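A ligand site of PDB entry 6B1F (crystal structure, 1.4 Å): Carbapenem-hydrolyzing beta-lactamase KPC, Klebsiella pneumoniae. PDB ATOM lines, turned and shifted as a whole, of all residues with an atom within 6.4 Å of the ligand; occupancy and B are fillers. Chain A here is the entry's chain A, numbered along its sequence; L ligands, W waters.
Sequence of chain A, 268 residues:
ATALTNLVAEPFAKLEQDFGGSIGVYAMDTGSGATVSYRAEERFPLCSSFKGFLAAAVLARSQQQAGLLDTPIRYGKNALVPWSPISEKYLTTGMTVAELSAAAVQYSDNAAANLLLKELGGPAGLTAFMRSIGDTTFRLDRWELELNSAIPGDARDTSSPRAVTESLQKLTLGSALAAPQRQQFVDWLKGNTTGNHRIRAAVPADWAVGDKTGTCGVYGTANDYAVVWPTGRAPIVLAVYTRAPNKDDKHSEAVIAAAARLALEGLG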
ATOM      1  N   LEU A  46      15.860  20.128  28.517  1.00  0.00           N
ATOM      2  CA  LEU A  46      15.741  21.574  28.717  1.00  0.00           C
ATOM      3  C   LEU A  46      16.981  22.304  28.261  1.00  0.00           C
ATOM      4  O   LEU A  46      16.877  23.440  27.788  1.00  0.00           O
ATOM      5  CB  LEU A  46      15.512  21.884  30.193  1.00  0.00           C
ATOM      6  CG  LEU A  46      14.109  21.510  30.686  1.00  0.00           C
ATOM      7  CD1 LEU A  46      14.080  21.310  32.180  1.00  0.00           C
ATOM      8  CD2 LEU A  46      13.079  22.545  30.246  1.00  0.00           C
ATOM      9  N   CYS A  47      18.158  21.723  28.477  1.00  0.00           N
ATOM     10  CA  CYS A  47      19.421  22.454  28.298  1.00  0.00           C
ATOM     11  C   CYS A  47      19.318  23.790  29.066  1.00  0.00           C
ATOM     12  O   CYS A  47      18.713  23.820  30.129  1.00  0.00           O
ATOM     13  CB  CYS A  47      19.735  22.659  26.813  1.00  0.00           C
ATOM     14  SG  CYS A  47      19.462  21.199  25.784  1.00  0.00           S
ATOM     15  N   SER A  48      19.863  24.888  28.524  1.00  0.00           N
ATOM     16  CA  SER A  48      19.828  26.200  29.195  1.00  0.00           C
ATOM     17  C   SER A  48      18.445  26.789  29.386  1.00  0.00           C
ATOM     18  O   SER A  48      18.325  27.776  30.097  1.00  0.00           O
ATOM     19  CB  SER A  48      20.603  27.245  28.401  1.00  0.00           C
ATOM     20  OG  SER A  48      21.993  27.032  28.399  1.00  0.00           O
ATOM     21  N   SER A  49      17.421  26.250  28.718  1.00  0.00           N
ATOM     22  CA  SER A  49      16.098  26.853  28.781  1.00  0.00           C
ATOM     23  C   SER A  49      15.473  26.810  30.171  1.00  0.00           C
ATOM     24  O   SER A  49      14.561  27.588  30.464  1.00  0.00           O
ATOM     25  CB  SER A  49      15.139  26.275  27.738  1.00  0.00           C
ATOM     26  OG  SER A  49      14.691  24.970  28.035  1.00  0.00           O
ATOM     27  N   LYS A  51      16.656  28.133  32.624  1.00  0.00           N
ATOM     28  CA  LYS A  51      17.083  29.363  33.314  1.00  0.00           C
ATOM     29  C   LYS A  51      15.997  30.435  33.355  1.00  0.00           C
ATOM     30  O   LYS A  51      15.981  31.235  34.274  1.00  0.00           O
ATOM     31  CB  LYS A  51      18.373  29.897  32.709  1.00  0.00           C
ATOM     32  CG  LYS A  51      19.572  28.987  32.936  1.00  0.00           C
ATOM     33  CD  LYS A  51      20.760  29.318  32.047  1.00  0.00           C
ATOM     34  CE  LYS A  51      21.848  28.274  32.222  1.00  0.00           C
ATOM     35  NZ  LYS A  51      22.908  28.348  31.189  1.00  0.00           N
ATOM     36  N   PRO A  82      32.655  27.131  32.290  1.00  0.00           N
ATOM     37  CA  PRO A  82      32.553  27.706  30.959  1.00  0.00           C
ATOM     38  C   PRO A  82      31.145  28.202  30.616  1.00  0.00           C
ATOM     39  O   PRO A  82      30.157  27.713  31.180  1.00  0.00           O
ATOM     40  CB  PRO A  82      32.993  26.567  30.034  1.00  0.00           C
ATOM     41  CG  PRO A  82      33.850  25.711  30.917  1.00  0.00           C
ATOM     42  CD  PRO A  82      33.202  25.757  32.251  1.00  0.00           C
ATOM     43  N   TRP A  83      31.062  29.182  29.719  1.00  0.00           N
ATOM     44  CA  TRP A  83      29.805  29.862  29.351  1.00  0.00           C
ATOM     45  C   TRP A  83      29.201  30.558  30.564  1.00  0.00           C
ATOM     46  O   TRP A  83      27.977  30.445  30.833  1.00  0.00           O
ATOM     47  CB  TRP A  83      28.812  28.929  28.651  1.00  0.00           C
ATOM     48  CG  TRP A  83      29.269  28.388  27.326  1.00  0.00           C
ATOM     49  CD1 TRP A  83      29.183  28.999  26.108  1.00  0.00           C
ATOM     50  CD2 TRP A  83      29.825  27.093  27.097  1.00  0.00           C
ATOM     51  NE1 TRP A  83      29.687  28.161  25.123  1.00  0.00           N
ATOM     52  CE2 TRP A  83      30.089  26.987  25.708  1.00  0.00           C
ATOM     53  CE3 TRP A  83      30.158  26.008  27.918  1.00  0.00           C
ATOM     54  CZ2 TRP A  83      30.642  25.839  25.125  1.00  0.00           C
ATOM     55  CZ3 TRP A  83      30.710  24.860  27.336  1.00  0.00           C
ATOM     56  CH2 TRP A  83      30.936  24.791  25.949  1.00  0.00           C
ATOM     57  N   TYR A 107      22.076  36.033  28.952  1.00  0.00           N
ATOM     58  CA  TYR A 107      23.364  35.519  28.442  1.00  0.00           C
ATOM     59  C   TYR A 107      23.509  34.034  28.705  1.00  0.00           C
ATOM     60  O   TYR A 107      24.530  33.458  28.386  1.00  0.00           O
ATOM     61  CB  TYR A 107      24.536  36.310  29.060  1.00  0.00           C
ATOM     62  CG  TYR A 107      24.547  37.721  28.556  1.00  0.00           C
ATOM     63  CD1 TYR A 107      25.198  38.038  27.375  1.00  0.00           C
ATOM     64  CD2 TYR A 107      23.873  38.718  29.229  1.00  0.00           C
ATOM     65  CE1 TYR A 107      25.199  39.336  26.875  1.00  0.00           C
ATOM     66  CE2 TYR A 107      23.859  40.037  28.741  1.00  0.00           C
ATOM     67  CZ  TYR A 107      24.529  40.318  27.565  1.00  0.00           C
ATOM     68  OH  TYR A 107      24.530  41.594  27.071  1.00  0.00           O
ATOM     69  N   SER A 108      22.508  33.406  29.301  1.00  0.00           N
ATOM     70  CA  SER A 108      22.558  31.978  29.581  1.00  0.00           C
ATOM     71  C   SER A 108      23.768  31.629  30.453  1.00  0.00           C
ATOM     72  O   SER A 108      24.357  30.555  30.328  1.00  0.00           O
ATOM     73  CB  SER A 108      22.533  31.181  28.283  1.00  0.00           C
ATOM     74  OG  SER A 108      21.789  30.011  28.449  1.00  0.00           O
ATOM     75  N   ASP A 109      24.091  32.517  31.383  1.00  0.00           N
ATOM     76  CA  ASP A 109      25.278  32.389  32.215  1.00  0.00           C
ATOM     77  C   ASP A 109      25.166  31.162  33.126  1.00  0.00           C
ATOM     78  O   ASP A 109      24.270  31.069  33.952  1.00  0.00           O
ATOM     79  CB  ASP A 109      25.439  33.673  33.038  1.00  0.00           C
ATOM     80  CG  ASP A 109      26.767  33.788  33.720  1.00  0.00           C
ATOM     81  OD1 ASP A 109      27.533  34.716  33.348  1.00  0.00           O
ATOM     82  OD2 ASP A 109      27.058  33.010  34.653  1.00  0.00           O
ATOM     83  N   ASN A 110      26.088  30.220  32.960  1.00  0.00           N
ATOM     84  CA  ASN A 110      26.002  28.935  33.680  1.00  0.00           C
ATOM     85  C   ASN A 110      26.260  29.063  35.183  1.00  0.00           C
ATOM     86  O   ASN A 110      25.517  28.528  35.996  1.00  0.00           O
ATOM     87  CB  ASN A 110      26.990  27.899  33.103  1.00  0.00           C
ATOM     88  CG  ASN A 110      26.480  27.194  31.862  1.00  0.00           C
ATOM     89  OD1 ASN A 110      25.286  27.136  31.587  1.00  0.00           O
ATOM     90  ND2 ASN A 110      27.415  26.622  31.102  1.00  0.00           N
ATOM     91  N   GLU A 144      24.579  22.724  36.196  1.00  0.00           N
ATOM     92  CA  GLU A 144      25.446  23.013  35.050  1.00  0.00           C
ATOM     93  C   GLU A 144      26.835  22.455  35.360  1.00  0.00           C
ATOM     94  O   GLU A 144      27.333  22.673  36.459  1.00  0.00           O
ATOM     95  CB  GLU A 144      25.566  24.511  34.826  1.00  0.00           C
ATOM     96  CG  GLU A 144      24.317  25.183  34.288  1.00  0.00           C
ATOM     97  CD  GLU A 144      23.960  24.773  32.887  1.00  0.00           C
ATOM     98  OE1 GLU A 144      24.702  24.006  32.242  1.00  0.00           O
ATOM     99  OE2 GLU A 144      22.927  25.256  32.405  1.00  0.00           O
ATOM    100  N   LEU A 145      27.497  21.762  34.434  1.00  0.00           N
ATOM    101  CA  LEU A 145      27.087  21.558  33.033  1.00  0.00           C
ATOM    102  C   LEU A 145      26.520  20.156  32.752  1.00  0.00           C
ATOM    103  O   LEU A 145      26.161  19.846  31.621  1.00  0.00           O
ATOM    104  CB  LEU A 145      28.261  21.862  32.087  1.00  0.00           C
ATOM    105  CG  LEU A 145      28.603  23.335  31.831  1.00  0.00           C
ATOM    106  CD1 LEU A 145      29.339  23.958  33.011  1.00  0.00           C
ATOM    107  CD2 LEU A 145      29.440  23.456  30.573  1.00  0.00           C
ATOM    108  N   LEU A 147      23.753  18.775  33.296  1.00  0.00           N
ATOM    109  CA  LEU A 147      22.376  18.724  32.802  1.00  0.00           C
ATOM    110  C   LEU A 147      22.238  18.808  31.271  1.00  0.00           C
ATOM    111  O   LEU A 147      21.163  18.560  30.746  1.00  0.00           O
ATOM    112  CB  LEU A 147      21.522  19.806  33.487  1.00  0.00           C
ATOM    113  CG  LEU A 147      21.879  21.279  33.215  1.00  0.00           C
ATOM    114  CD1 LEU A 147      21.315  21.825  31.900  1.00  0.00           C
ATOM    115  CD2 LEU A 147      21.398  22.175  34.351  1.00  0.00           C
ATOM    116  N   ASN A 148      23.326  19.156  30.589  1.00  0.00           N
ATOM    117  CA  ASN A 148      23.336  19.292  29.118  1.00  0.00           C
ATOM    118  C   ASN A 148      23.604  17.992  28.376  1.00  0.00           C
ATOM    119  O   ASN A 148      23.705  17.999  27.144  1.00  0.00           O
ATOM    120  CB  ASN A 148      24.352  20.340  28.688  1.00  0.00           C
ATOM    121  CG  ASN A 148      24.045  21.694  29.260  1.00  0.00           C
ATOM    122  OD1 ASN A 148      23.079  22.348  28.845  1.00  0.00           O
ATOM    123  ND2 ASN A 148      24.827  22.123  30.227  1.00  0.00           N
ATOM    124  N   ASN A 192      16.615  39.302  26.227  1.00  0.00           N
ATOM    125  CA  ASN A 192      17.507  38.199  25.864  1.00  0.00           C
ATOM    126  C   ASN A 192      18.367  38.543  24.658  1.00  0.00           C
ATOM    127  O   ASN A 192      17.909  39.172  23.701  1.00  0.00           O
ATOM    128  CB  ASN A 192      16.735  36.931  25.574  1.00  0.00           C
ATOM    129  CG  ASN A 192      17.645  35.776  25.244  1.00  0.00           C
ATOM    130  OD1 ASN A 192      18.720  35.655  25.843  1.00  0.00           O
ATOM    131  ND2 ASN A 192      17.261  34.948  24.276  1.00  0.00           N
ATOM    132  N   THR A 194      20.457  36.009  23.180  1.00  0.00           N
ATOM    133  CA  THR A 194      20.907  34.774  22.556  1.00  0.00           C
ATOM    134  C   THR A 194      19.929  34.182  21.549  1.00  0.00           C
ATOM    135  O   THR A 194      20.224  33.151  20.938  1.00  0.00           O
ATOM    136  CB  THR A 194      21.162  33.674  23.622  1.00  0.00           C
ATOM    137  OG1 THR A 194      19.912  33.289  24.177  1.00  0.00           O
ATOM    138  CG2 THR A 194      22.102  34.154  24.699  1.00  0.00           C
ATOM    139  N   GLY A 195      18.775  34.829  21.344  1.00  0.00           N
ATOM    140  CA  GLY A 195      17.670  34.240  20.592  1.00  0.00           C
ATOM    141  C   GLY A 195      17.376  34.821  19.211  1.00  0.00           C
ATOM    142  O   GLY A 195      16.342  34.512  18.643  1.00  0.00           O
ATOM    143  N   ARG A 198      16.343  32.318  16.290  1.00  0.00           N
ATOM    144  CA  ARG A 198      15.380  31.267  16.635  1.00  0.00           C
ATOM    145  C   ARG A 198      13.973  31.824  16.496  1.00  0.00           C
ATOM    146  O   ARG A 198      13.628  32.304  15.401  1.00  0.00           O
ATOM    147  CB  ARG A 198      15.751  30.639  17.975  1.00  0.00           C
ATOM    148  CG  ARG A 198      17.077  29.919  17.868  1.00  0.00           C
ATOM    149  CD  ARG A 198      17.461  29.163  19.113  1.00  0.00           C
ATOM    150  NE  ARG A 198      18.866  28.760  19.010  1.00  0.00           N
ATOM    151  CZ  ARG A 198      19.513  27.956  19.839  1.00  0.00           C
ATOM    152  NH1 ARG A 198      18.890  27.348  20.842  1.00  0.00           N
ATOM    153  NH2 ARG A 198      20.815  27.711  19.619  1.00  0.00           N
ATOM    154  N   LYS A 212      13.738  32.555  25.792  1.00  0.00           N
ATOM    155  CA  LYS A 212      14.900  31.900  26.377  1.00  0.00           C
ATOM    156  C   LYS A 212      15.280  30.703  25.536  1.00  0.00           C
ATOM    157  O   LYS A 212      14.434  29.867  25.238  1.00  0.00           O
ATOM    158  CB  LYS A 212      14.613  31.452  27.808  1.00  0.00           C
ATOM    159  CG  LYS A 212      15.771  30.742  28.511  1.00  0.00           C
ATOM    160  CD  LYS A 212      16.846  31.709  28.971  1.00  0.00           C
ATOM    161  CE  LYS A 212      18.195  31.011  29.191  1.00  0.00           C
ATOM    162  NZ  LYS A 212      18.982  30.751  27.966  1.00  0.00           N
ATOM    163  N   THR A 213      16.576  30.607  25.205  1.00  0.00           N
ATOM    164  CA  THR A 213      17.108  29.532  24.386  1.00  0.00           C
ATOM    165  C   THR A 213      17.792  28.461  25.217  1.00  0.00           C
ATOM    166  O   THR A 213      18.111  28.651  26.417  1.00  0.00           O
ATOM    167  CB  THR A 213      18.144  30.093  23.429  1.00  0.00           C
ATOM    168  OG1 THR A 213      19.169  30.739  24.182  1.00  0.00           O
ATOM    169  CG2 THR A 213      17.522  31.089  22.501  1.00  0.00           C
ATOM    170  N   GLY A 214      18.012  27.319  24.558  1.00  0.00           N
ATOM    171  CA  GLY A 214      18.812  26.231  25.111  1.00  0.00           C
ATOM    172  C   GLY A 214      19.585  25.534  24.001  1.00  0.00           C
ATOM    173  O   GLY A 214      19.044  25.340  22.924  1.00  0.00           O
ATOM    174  N   THR A 215      20.834  25.169  24.261  1.00  0.00           N
ATOM    175  CA  THR A 215      21.653  24.492  23.262  1.00  0.00           C
ATOM    176  C   THR A 215      22.553  23.494  23.990  1.00  0.00           C
ATOM    177  O   THR A 215      23.585  23.871  24.479  1.00  0.00           O
ATOM    178  CB  THR A 215      22.510  25.511  22.464  1.00  0.00           C
ATOM    179  OG1 THR A 215      21.713  26.622  22.048  1.00  0.00           O
ATOM    180  CG2 THR A 215      23.131  24.819  21.268  1.00  0.00           C
ATOM    181  N   CYS A 216      22.151  22.236  24.063  1.00  0.00           N
ATOM    182  CA  CYS A 216      22.914  21.242  24.853  1.00  0.00           C
ATOM    183  C   CYS A 216      24.303  20.941  24.322  1.00  0.00           C
ATOM    184  O   CYS A 216      25.186  20.568  25.108  1.00  0.00           O
ATOM    185  CB  CYS A 216      22.147  19.919  24.975  1.00  0.00           C
ATOM    186  SG  CYS A 216      20.953  19.879  26.319  1.00  0.00           S
ATOM    187  N   GLY A 217      24.498  21.090  23.018  1.00  0.00           N
ATOM    188  CA  GLY A 217      25.803  20.889  22.380  1.00  0.00           C
ATOM    189  C   GLY A 217      26.030  19.494  21.836  1.00  0.00           C
ATOM    190  O   GLY A 217      27.143  19.162  21.408  1.00  0.00           O
ATOM    191  N   ASN A 223      16.711  24.437  21.608  1.00  0.00           N
ATOM    192  CA  ASN A 223      15.336  24.860  21.838  1.00  0.00           C
ATOM    193  C   ASN A 223      15.210  26.360  22.034  1.00  0.00           C
ATOM    194  O   ASN A 223      16.194  27.075  22.138  1.00  0.00           O
ATOM    195  CB  ASN A 223      14.768  24.089  23.028  1.00  0.00           C
ATOM    196  CG  ASN A 223      15.623  24.221  24.261  1.00  0.00           C
ATOM    197  OD1 ASN A 223      15.811  25.307  24.767  1.00  0.00           O
ATOM    198  ND2 ASN A 223      16.140  23.104  24.765  1.00  0.00           N
HETATM  199  O1  LIG L   1      22.146  30.591  24.711  1.00  0.00           O
HETATM  200  S1  LIG L   1      22.218  29.123  24.808  1.00  0.00           S
HETATM  201  O2  LIG L   1      21.605  28.484  23.644  1.00  0.00           O
HETATM  202  O3  LIG L   1      21.485  28.749  25.991  1.00  0.00           O
HETATM  203  O4  LIG L   1      23.682  28.625  24.909  1.00  0.00           O
HETATM  204  N1  LIG L   1      24.671  29.191  25.784  1.00  0.00           N
HETATM  205  C1  LIG L   1      25.578  28.442  26.710  1.00  0.00           C
HETATM  206  C2  LIG L   1      26.253  27.371  25.786  1.00  0.00           C
HETATM  207  C3  LIG L   1      25.448  26.056  25.506  1.00  0.00           C
HETATM  208  C4  LIG L   1      24.957  25.448  26.790  1.00  0.00           C
HETATM  209  C5  LIG L   1      25.828  25.077  27.878  1.00  0.00           C
HETATM  210  N2  LIG L   1      26.531  24.781  28.761  1.00  0.00           N
HETATM  211  N3  LIG L   1      24.015  26.549  27.358  1.00  0.00           N
HETATM  212  C6  LIG L   1      22.722  26.283  27.577  1.00  0.00           C
HETATM  213  O5  LIG L   1      22.020  25.406  26.941  1.00  0.00           O
HETATM  214  C7  LIG L   1      24.585  27.871  27.725  1.00  0.00           C
HETATM  215  O   HOH W   1      22.897  24.782  29.901  1.00  0.00           O
HETATM  216  O   HOH W   2      20.744  30.365  21.420  1.00  0.00           O
HETATM  217  O   HOH W   3      25.818  31.450  24.498  1.00  0.00           O
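Water W2 lies within hydrogen-bond range of O of Thr 194 (2.9 Å), O2 of the ligand (3.0 Å), OG1 of Thr 213 (3.2 Å) and NH2 of Arg 198 (3.2 Å).
The backbone NH of Ser 48 lies within hydrogen-bond range of an oxygen (O5) of the ligand (2.7 Å).
OG of Ser 48 is covalently linked to C6 of the ligand (1.3 Å).
O5 of the ligand lies within hydrogen-bond range of N of Thr 215.
O2 of the ligand lies within hydrogen-bond range of OG1 of Thr 215.
OG of Ser 108 sits at hydrogen-bond distance from O3 of the ligand (2.8 Å).
The side-chain hydroxyl (OG1) of Thr 213 sits at hydrogen-bond distance from an oxygen (O1) of the ligand (3.0 Å).
The side-chain amide nitrogen (ND2) of Asn 110 lies within hydrogen-bond range of a nitrogen (N2) of the ligand, 3.1 Å away.
ND2 of Asn 148 lies within hydrogen-bond range of N2 of the ligand (3.5 Å).
O3 of the ligand is in salt-bridge range of NZ of Lys 212 (3.8 Å).
CB of Cys 47 touches O5 of the ligand (3.6 Å).
Lys 51 touches the ligand (NZ to C7, 3.9 Å).
Trp 83 touches the ligand.
CD2 of Leu 145 touches N2 of the ligand, 3.7 Å away.
CB of Thr 194 touches O1 of the ligand, 3.4 Å away.
C of Gly 214 touches O2 of the ligand (3.6 Å).
Hydrophobic or aromatic side chains within 4 Å of the ligand: Trp 83 and Leu 145.
13 residues have an atom within 4 Å of the ligand: Cys 47, Ser 48, Lys 51, Trp 83, Ser 108, Asn 110, Leu 145, Asn 148, Thr 194, Lys 212, Thr 213, Gly 214 and Thr 215.
OG of Ser 48 sits at hydrogen-bond distance from OG of Ser 108 (3.0 Å).
The guanidinium group (NH2) of Arg 198 lies within hydrogen-bond range of the side-chain hydroxyl (OG1) of Thr 215, 2.8 Å away.
The side-chain amino group of Lys 212 is in hydrogen-bond range of the side-chain hydroxyl of Ser 108.
The backbone NH (N) of Asn 110 is in hydrogen-bond range of the backbone carbonyl oxygen (O) of Trp 83 (2.9 Å).
The backbone carbonyl oxygen (O) of Leu 145 is in hydrogen-bond range of the side-chain amide nitrogen (ND2) of Asn 148 (3.0 Å).
SG of Cys 47 is disulfide-bonded to SG of Cys 216 (2.1 Å).
The backbone carbonyl oxygen (O) of Gly 214 lies within hydrogen-bond range of the guanidinium group (NH1) of Arg 198.
N of Asn 223 lies within hydrogen-bond range of O of Gly 214 (2.8 Å).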
